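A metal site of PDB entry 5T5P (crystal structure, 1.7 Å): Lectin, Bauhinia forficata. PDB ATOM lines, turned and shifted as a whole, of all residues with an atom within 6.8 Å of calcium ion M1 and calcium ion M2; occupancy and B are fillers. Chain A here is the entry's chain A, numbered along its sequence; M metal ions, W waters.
Water W4 bridges the side-chain carboxylate (OE1) of Glu 118 (2.6 Å) and the backbone carbonyl oxygen (O) of Ile 142 (2.8 Å).
Calcium ion M1 is bound by the side-chain amide oxygen (OD1) of Asn 124 (2.3 Å), water W1 (2.3 Å), the backbone carbonyl oxygen (O) of Trp 122 (2.4 Å), the side-chain carboxylate (OE2) of Glu 129 (2.4 Å), water W3 (2.5 Å), the side-chain carboxylate (OD2) of Asp 120 (2.5 Å) and the side-chain carboxylate (OD1) of Asp 120 (2.5 Å).
Four residues have an atom within 4 Å of calcium ion M1: Asp 120, Trp 122, Asn 124 and Glu 129. The nearest printed residue that does not touch calcium ion M1 is Val 123 (4.5 Å).
Calcium ion M2 is bound by the side-chain carboxylate (OD2) of Asp 120 (2.2 Å), water W2 (2.3 Å), water W4 (2.3 Å), the side-chain carboxylate (OE2) of Glu 118 (2.3 Å), the side-chain carboxylate (OE1) of Glu 129 (2.3 Å) and a ring nitrogen (NE2) of His 134 (2.4 Å). Calcium ion M2 has six donor atoms within binding distance.
Within 4 Å of calcium ion M2: Glu 118, Asp 120, Glu 129 and His 134. The nearest printed residue that does not touch calcium ion M2 is Ser 144 (4.3 Å).
The side-chain carboxylate (OD2) of Asp 138 lies close to the side-chain carboxylate (OE1) of Glu 118. N of Glu 118 is in hydrogen-bond range of O of Gly 136. The side-chain carboxylate (OE1) of Glu 129 lies close to the indole nitrogen (NE1) of Trp 127 (3.1 Å).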
ATOM      1  N   ASP A  78     -25.184 -10.557 -17.877  1.00  0.00           N
ATOM      2  CA  ASP A  78     -23.726 -10.470 -17.671  1.00  0.00           C
ATOM      3  C   ASP A  78     -23.027  -9.373 -18.345  1.00  0.00           C
ATOM      4  O   ASP A  78     -21.877  -9.086 -18.070  1.00  0.00           O
ATOM      5  CB  ASP A  78     -23.069 -11.821 -18.035  1.00  0.00           C
ATOM      6  CG  ASP A  78     -23.267 -12.816 -16.937  1.00  0.00           C
ATOM      7  OD1 ASP A  78     -22.410 -12.782 -15.994  1.00  0.00           O
ATOM      8  OD2 ASP A  78     -24.281 -13.605 -16.910  1.00  0.00           O
ATOM      9  N   GLY A  95     -23.913 -16.711 -19.503  1.00  0.00           N
ATOM     10  CA  GLY A  95     -23.346 -16.283 -18.219  1.00  0.00           C
ATOM     11  C   GLY A  95     -22.083 -15.461 -18.429  1.00  0.00           C
ATOM     12  O   GLY A  95     -21.959 -14.683 -19.412  1.00  0.00           O
ATOM     13  N   GLY A  96     -21.195 -15.523 -17.433  1.00  0.00           N
ATOM     14  CA  GLY A  96     -20.020 -14.647 -17.423  1.00  0.00           C
ATOM     15  C   GLY A  96     -18.992 -14.870 -18.518  1.00  0.00           C
ATOM     16  O   GLY A  96     -18.174 -14.002 -18.738  1.00  0.00           O
ATOM     17  N   TYR A  97     -19.218 -15.881 -19.360  1.00  0.00           N
ATOM     18  CA  TYR A  97     -18.403 -16.170 -20.529  1.00  0.00           C
ATOM     19  C   TYR A  97     -18.775 -15.236 -21.722  1.00  0.00           C
ATOM     20  O   TYR A  97     -18.048 -15.175 -22.670  1.00  0.00           O
ATOM     21  CB  TYR A  97     -18.505 -17.635 -20.921  1.00  0.00           C
ATOM     22  CG  TYR A  97     -18.091 -18.533 -19.784  1.00  0.00           C
ATOM     23  CD1 TYR A  97     -16.753 -18.659 -19.468  1.00  0.00           C
ATOM     24  CD2 TYR A  97     -19.032 -19.181 -19.013  1.00  0.00           C
ATOM     25  CE1 TYR A  97     -16.340 -19.410 -18.365  1.00  0.00           C
ATOM     26  CE2 TYR A  97     -18.683 -19.911 -17.870  1.00  0.00           C
ATOM     27  CZ  TYR A  97     -17.334 -20.070 -17.575  1.00  0.00           C
ATOM     28  OH  TYR A  97     -16.958 -20.845 -16.465  1.00  0.00           O
ATOM     29  N   LEU A  98     -19.888 -14.487 -21.543  1.00  0.00           N
ATOM     30  CA  LEU A  98     -20.267 -13.407 -22.466  1.00  0.00           C
ATOM     31  C   LEU A  98     -20.483 -13.859 -23.858  1.00  0.00           C
ATOM     32  O   LEU A  98     -20.467 -13.051 -24.782  1.00  0.00           O
ATOM     33  CB  LEU A  98     -19.304 -12.200 -22.444  1.00  0.00           C
ATOM     34  CG  LEU A  98     -19.232 -11.475 -21.118  1.00  0.00           C
ATOM     35  CD1 LEU A  98     -18.114 -10.434 -21.073  1.00  0.00           C
ATOM     36  CD2 LEU A  98     -20.494 -10.747 -20.785  1.00  0.00           C
ATOM     37  N   GLU A 118     -15.250  -5.495 -23.658  1.00  0.00           N
ATOM     38  CA  GLU A 118     -16.357  -5.991 -22.878  1.00  0.00           C
ATOM     39  C   GLU A 118     -16.935  -4.917 -21.978  1.00  0.00           C
ATOM     40  O   GLU A 118     -16.179  -4.066 -21.414  1.00  0.00           O
ATOM     41  CB  GLU A 118     -15.975  -7.264 -22.120  1.00  0.00           C
ATOM     42  CG  GLU A 118     -14.970  -7.037 -21.030  1.00  0.00           C
ATOM     43  CD  GLU A 118     -14.863  -8.212 -20.055  1.00  0.00           C
ATOM     44  OE1 GLU A 118     -14.671  -9.368 -20.500  1.00  0.00           O
ATOM     45  OE2 GLU A 118     -14.885  -7.944 -18.865  1.00  0.00           O
ATOM     46  N   ASP A 120     -19.060  -5.263 -18.720  1.00  0.00           N
ATOM     47  CA  ASP A 120     -19.258  -6.392 -17.780  1.00  0.00           C
ATOM     48  C   ASP A 120     -20.069  -5.955 -16.584  1.00  0.00           C
ATOM     49  O   ASP A 120     -19.603  -5.161 -15.740  1.00  0.00           O
ATOM     50  CB  ASP A 120     -17.899  -6.964 -17.395  1.00  0.00           C
ATOM     51  CG  ASP A 120     -18.006  -8.250 -16.685  1.00  0.00           C
ATOM     52  OD1 ASP A 120     -19.068  -8.507 -16.041  1.00  0.00           O
ATOM     53  OD2 ASP A 120     -17.054  -9.084 -16.665  1.00  0.00           O
ATOM     54  N   THR A 121     -21.329  -6.429 -16.490  1.00  0.00           N
ATOM     55  CA  THR A 121     -22.239  -6.011 -15.489  1.00  0.00           C
ATOM     56  C   THR A 121     -22.269  -6.924 -14.241  1.00  0.00           C
ATOM     57  O   THR A 121     -22.920  -6.532 -13.248  1.00  0.00           O
ATOM     58  CB  THR A 121     -23.695  -5.946 -15.955  1.00  0.00           C
ATOM     59  OG1 THR A 121     -24.061  -7.251 -16.491  1.00  0.00           O
ATOM     60  CG2 THR A 121     -23.853  -4.981 -17.064  1.00  0.00           C
ATOM     61  N   TRP A 122     -21.536  -8.039 -14.250  1.00  0.00           N
ATOM     62  CA  TRP A 122     -21.609  -8.975 -13.140  1.00  0.00           C
ATOM     63  C   TRP A 122     -20.208  -9.400 -12.706  1.00  0.00           C
ATOM     64  O   TRP A 122     -19.460  -9.922 -13.494  1.00  0.00           O
ATOM     65  CB  TRP A 122     -22.412 -10.225 -13.531  1.00  0.00           C
ATOM     66  CG  TRP A 122     -22.415 -11.278 -12.460  1.00  0.00           C
ATOM     67  CD1 TRP A 122     -21.437 -12.212 -12.237  1.00  0.00           C
ATOM     68  CD2 TRP A 122     -23.419 -11.514 -11.468  1.00  0.00           C
ATOM     69  NE1 TRP A 122     -21.781 -12.987 -11.134  1.00  0.00           N
ATOM     70  CE2 TRP A 122     -22.974 -12.562 -10.655  1.00  0.00           C
ATOM     71  CE3 TRP A 122     -24.589 -10.879 -11.142  1.00  0.00           C
ATOM     72  CZ2 TRP A 122     -23.737 -13.069  -9.636  1.00  0.00           C
ATOM     73  CZ3 TRP A 122     -25.341 -11.337 -10.128  1.00  0.00           C
ATOM     74  CH2 TRP A 122     -24.913 -12.416  -9.342  1.00  0.00           C
ATOM     75  N   VAL A 123     -19.903  -9.125 -11.445  1.00  0.00           N
ATOM     76  CA  VAL A 123     -18.597  -9.472 -10.918  1.00  0.00           C
ATOM     77  C   VAL A 123     -18.530 -10.996 -10.653  1.00  0.00           C
ATOM     78  O   VAL A 123     -19.256 -11.575  -9.785  1.00  0.00           O
ATOM     79  CB  VAL A 123     -18.311  -8.700  -9.631  1.00  0.00           C
ATOM     80  CG1 VAL A 123     -17.039  -9.219  -8.943  1.00  0.00           C
ATOM     81  CG2 VAL A 123     -18.271  -7.181  -9.938  1.00  0.00           C
ATOM     82  N   ASN A 124     -17.752 -11.655 -11.510  1.00  0.00           N
ATOM     83  CA  ASN A 124     -17.567 -13.076 -11.413  1.00  0.00           C
ATOM     84  C   ASN A 124     -16.510 -13.437 -10.355  1.00  0.00           C
ATOM     85  O   ASN A 124     -15.478 -12.826 -10.308  1.00  0.00           O
ATOM     86  CB  ASN A 124     -17.212 -13.719 -12.710  1.00  0.00           C
ATOM     87  CG  ASN A 124     -18.429 -13.782 -13.656  1.00  0.00           C
ATOM     88  OD1 ASN A 124     -18.654 -12.851 -14.442  1.00  0.00           O
ATOM     89  ND2 ASN A 124     -19.233 -14.815 -13.507  1.00  0.00           N
ATOM     90  N   TRP A 127     -13.266 -16.505 -11.889  1.00  0.00           N
ATOM     91  CA  TRP A 127     -11.993 -16.157 -12.526  1.00  0.00           C
ATOM     92  C   TRP A 127     -11.685 -14.770 -11.972  1.00  0.00           C
ATOM     93  O   TRP A 127     -12.558 -14.146 -11.316  1.00  0.00           O
ATOM     94  CB  TRP A 127     -11.963 -16.129 -14.063  1.00  0.00           C
ATOM     95  CG  TRP A 127     -13.051 -15.372 -14.664  1.00  0.00           C
ATOM     96  CD1 TRP A 127     -13.114 -14.005 -14.913  1.00  0.00           C
ATOM     97  CD2 TRP A 127     -14.285 -15.914 -15.059  1.00  0.00           C
ATOM     98  NE1 TRP A 127     -14.369 -13.713 -15.432  1.00  0.00           N
ATOM     99  CE2 TRP A 127     -15.087 -14.871 -15.547  1.00  0.00           C
ATOM    100  CE3 TRP A 127     -14.796 -17.227 -15.087  1.00  0.00           C
ATOM    101  CZ2 TRP A 127     -16.376 -15.079 -16.017  1.00  0.00           C
ATOM    102  CZ3 TRP A 127     -16.072 -17.440 -15.536  1.00  0.00           C
ATOM    103  CH2 TRP A 127     -16.824 -16.389 -16.067  1.00  0.00           C
ATOM    104  N   LYS A 128     -10.466 -14.317 -12.180  1.00  0.00           N
ATOM    105  CA  LYS A 128     -10.039 -13.018 -11.677  1.00  0.00           C
ATOM    106  C   LYS A 128     -10.684 -11.873 -12.440  1.00  0.00           C
ATOM    107  O   LYS A 128     -10.519 -11.802 -13.661  1.00  0.00           O
ATOM    108  CB  LYS A 128      -8.483 -12.871 -11.829  1.00  0.00           C
ATOM    109  CG  LYS A 128      -8.025 -11.435 -11.707  1.00  0.00           C
ATOM    110  CD  LYS A 128      -6.733 -11.145 -10.948  1.00  0.00           C
ATOM    111  CE  LYS A 128      -5.454 -11.593 -11.643  1.00  0.00           C
ATOM    112  NZ  LYS A 128      -5.519 -11.739 -13.124  1.00  0.00           N
ATOM    113  N   GLU A 129     -11.467 -11.063 -11.776  1.00  0.00           N
ATOM    114  CA  GLU A 129     -11.833  -9.814 -12.352  1.00  0.00           C
ATOM    115  C   GLU A 129     -12.083  -8.840 -11.248  1.00  0.00           C
ATOM    116  O   GLU A 129     -12.077  -9.233 -10.066  1.00  0.00           O
ATOM    117  CB  GLU A 129     -12.989  -9.940 -13.377  1.00  0.00           C
ATOM    118  CG  GLU A 129     -14.235 -10.564 -12.909  1.00  0.00           C
ATOM    119  CD  GLU A 129     -15.270 -10.589 -14.065  1.00  0.00           C
ATOM    120  OE1 GLU A 129     -14.870 -10.637 -15.214  1.00  0.00           O
ATOM    121  OE2 GLU A 129     -16.476 -10.511 -13.772  1.00  0.00           O
ATOM    122  N   PRO A 130     -12.174  -7.547 -11.580  1.00  0.00           N
ATOM    123  CA  PRO A 130     -12.361  -6.516 -10.523  1.00  0.00           C
ATOM    124  C   PRO A 130     -13.611  -6.702  -9.710  1.00  0.00           C
ATOM    125  O   PRO A 130     -14.526  -7.274 -10.148  1.00  0.00           O
ATOM    126  CB  PRO A 130     -12.476  -5.200 -11.300  1.00  0.00           C
ATOM    127  CG  PRO A 130     -11.982  -5.478 -12.648  1.00  0.00           C
ATOM    128  CD  PRO A 130     -12.031  -6.948 -12.936  1.00  0.00           C
ATOM    129  N   HIS A 134     -17.238  -3.217 -14.750  1.00  0.00           N
ATOM    130  CA  HIS A 134     -16.077  -2.783 -15.472  1.00  0.00           C
ATOM    131  C   HIS A 134     -16.179  -2.898 -16.971  1.00  0.00           C
ATOM    132  O   HIS A 134     -16.995  -3.647 -17.486  1.00  0.00           O
ATOM    133  CB  HIS A 134     -14.826  -3.577 -14.981  1.00  0.00           C
ATOM    134  CG  HIS A 134     -14.984  -5.042 -15.014  1.00  0.00           C
ATOM    135  ND1 HIS A 134     -15.651  -5.758 -14.056  1.00  0.00           N
ATOM    136  CD2 HIS A 134     -14.607  -5.941 -15.955  1.00  0.00           C
ATOM    137  CE1 HIS A 134     -15.652  -7.034 -14.361  1.00  0.00           C
ATOM    138  NE2 HIS A 134     -15.026  -7.181 -15.509  1.00  0.00           N
ATOM    139  N   GLY A 136     -13.530  -3.605 -20.231  1.00  0.00           N
ATOM    140  CA  GLY A 136     -12.263  -4.316 -20.376  1.00  0.00           C
ATOM    141  C   GLY A 136     -11.910  -4.593 -21.819  1.00  0.00           C
ATOM    142  O   GLY A 136     -12.762  -4.669 -22.702  1.00  0.00           O
ATOM    143  N   ASP A 138     -10.189  -7.635 -23.848  1.00  0.00           N
ATOM    144  CA  ASP A 138      -9.920  -9.077 -23.685  1.00  0.00           C
ATOM    145  C   ASP A 138      -9.147  -9.532 -24.887  1.00  0.00           C
ATOM    146  O   ASP A 138      -9.543  -9.287 -26.027  1.00  0.00           O
ATOM    147  CB  ASP A 138     -11.219  -9.898 -23.580  1.00  0.00           C
ATOM    148  CG  ASP A 138     -12.131  -9.452 -22.492  1.00  0.00           C
ATOM    149  OD1 ASP A 138     -11.628  -8.868 -21.495  1.00  0.00           O
ATOM    150  OD2 ASP A 138     -13.347  -9.831 -22.536  1.00  0.00           O
ATOM    151  N   ILE A 142     -11.082 -14.550 -20.972  1.00  0.00           N
ATOM    152  CA  ILE A 142     -12.099 -13.809 -20.192  1.00  0.00           C
ATOM    153  C   ILE A 142     -11.511 -12.967 -19.052  1.00  0.00           C
ATOM    154  O   ILE A 142     -12.203 -12.101 -18.595  1.00  0.00           O
ATOM    155  CB  ILE A 142     -13.162 -14.767 -19.645  1.00  0.00           C
ATOM    156  CG1 ILE A 142     -14.466 -14.076 -19.258  1.00  0.00           C
ATOM    157  CG2 ILE A 142     -12.682 -15.591 -18.451  1.00  0.00           C
ATOM    158  CD1 ILE A 142     -15.256 -13.419 -20.381  1.00  0.00           C
ATOM    159  N   VAL A 143     -10.257 -13.165 -18.709  1.00  0.00           N
ATOM    160  CA  VAL A 143      -9.566 -12.286 -17.753  1.00  0.00           C
ATOM    161  C   VAL A 143      -8.939 -11.143 -18.598  1.00  0.00           C
ATOM    162  O   VAL A 143      -7.939 -11.368 -19.284  1.00  0.00           O
ATOM    163  CB  VAL A 143      -8.514 -13.058 -16.969  1.00  0.00           C
ATOM    164  CG1 VAL A 143      -7.748 -12.128 -16.041  1.00  0.00           C
ATOM    165  CG2 VAL A 143      -9.248 -14.113 -16.148  1.00  0.00           C
ATOM    166  N   SER A 144      -9.531 -10.000 -18.491  1.00  0.00           N
ATOM    167  CA  SER A 144      -9.127  -8.813 -19.276  1.00  0.00           C
ATOM    168  C   SER A 144      -7.666  -8.421 -19.103  1.00  0.00           C
ATOM    169  O   SER A 144      -7.073  -8.536 -17.985  1.00  0.00           O
ATOM    170  CB  SER A 144      -9.993  -7.631 -18.912  1.00  0.00           C
ATOM    171  OG  SER A 144     -11.384  -7.925 -19.102  1.00  0.00           O
ATOM    172  N   VAL A 147      -8.412  -3.234 -17.795  1.00  0.00           N
ATOM    173  CA  VAL A 147      -9.765  -3.082 -17.252  1.00  0.00           C
ATOM    174  C   VAL A 147      -9.904  -1.865 -16.435  1.00  0.00           C
ATOM    175  O   VAL A 147      -8.952  -1.480 -15.708  1.00  0.00           O
ATOM    176  CB  VAL A 147     -10.076  -4.419 -16.519  1.00  0.00           C
ATOM    177  CG1 VAL A 147      -9.236  -4.609 -15.238  1.00  0.00           C
ATOM    178  CG2 VAL A 147     -11.536  -4.559 -16.253  1.00  0.00           C
HETATM  179 CA    CA M   1     -18.291 -10.763 -15.355  1.00  0.00          CA
HETATM  180 CA    CA M   2     -14.877  -9.099 -16.901  1.00  0.00          CA
HETATM  181  O   HOH W   1     -20.340 -11.073 -16.447  1.00  0.00           O
HETATM  182  O   HOH W   2     -12.661  -8.696 -16.892  1.00  0.00           O
HETATM  183  O   HOH W   3     -17.210 -12.038 -17.155  1.00  0.00           O
HETATM  184  O   HOH W   4     -14.725 -10.837 -18.345  1.00  0.00           O
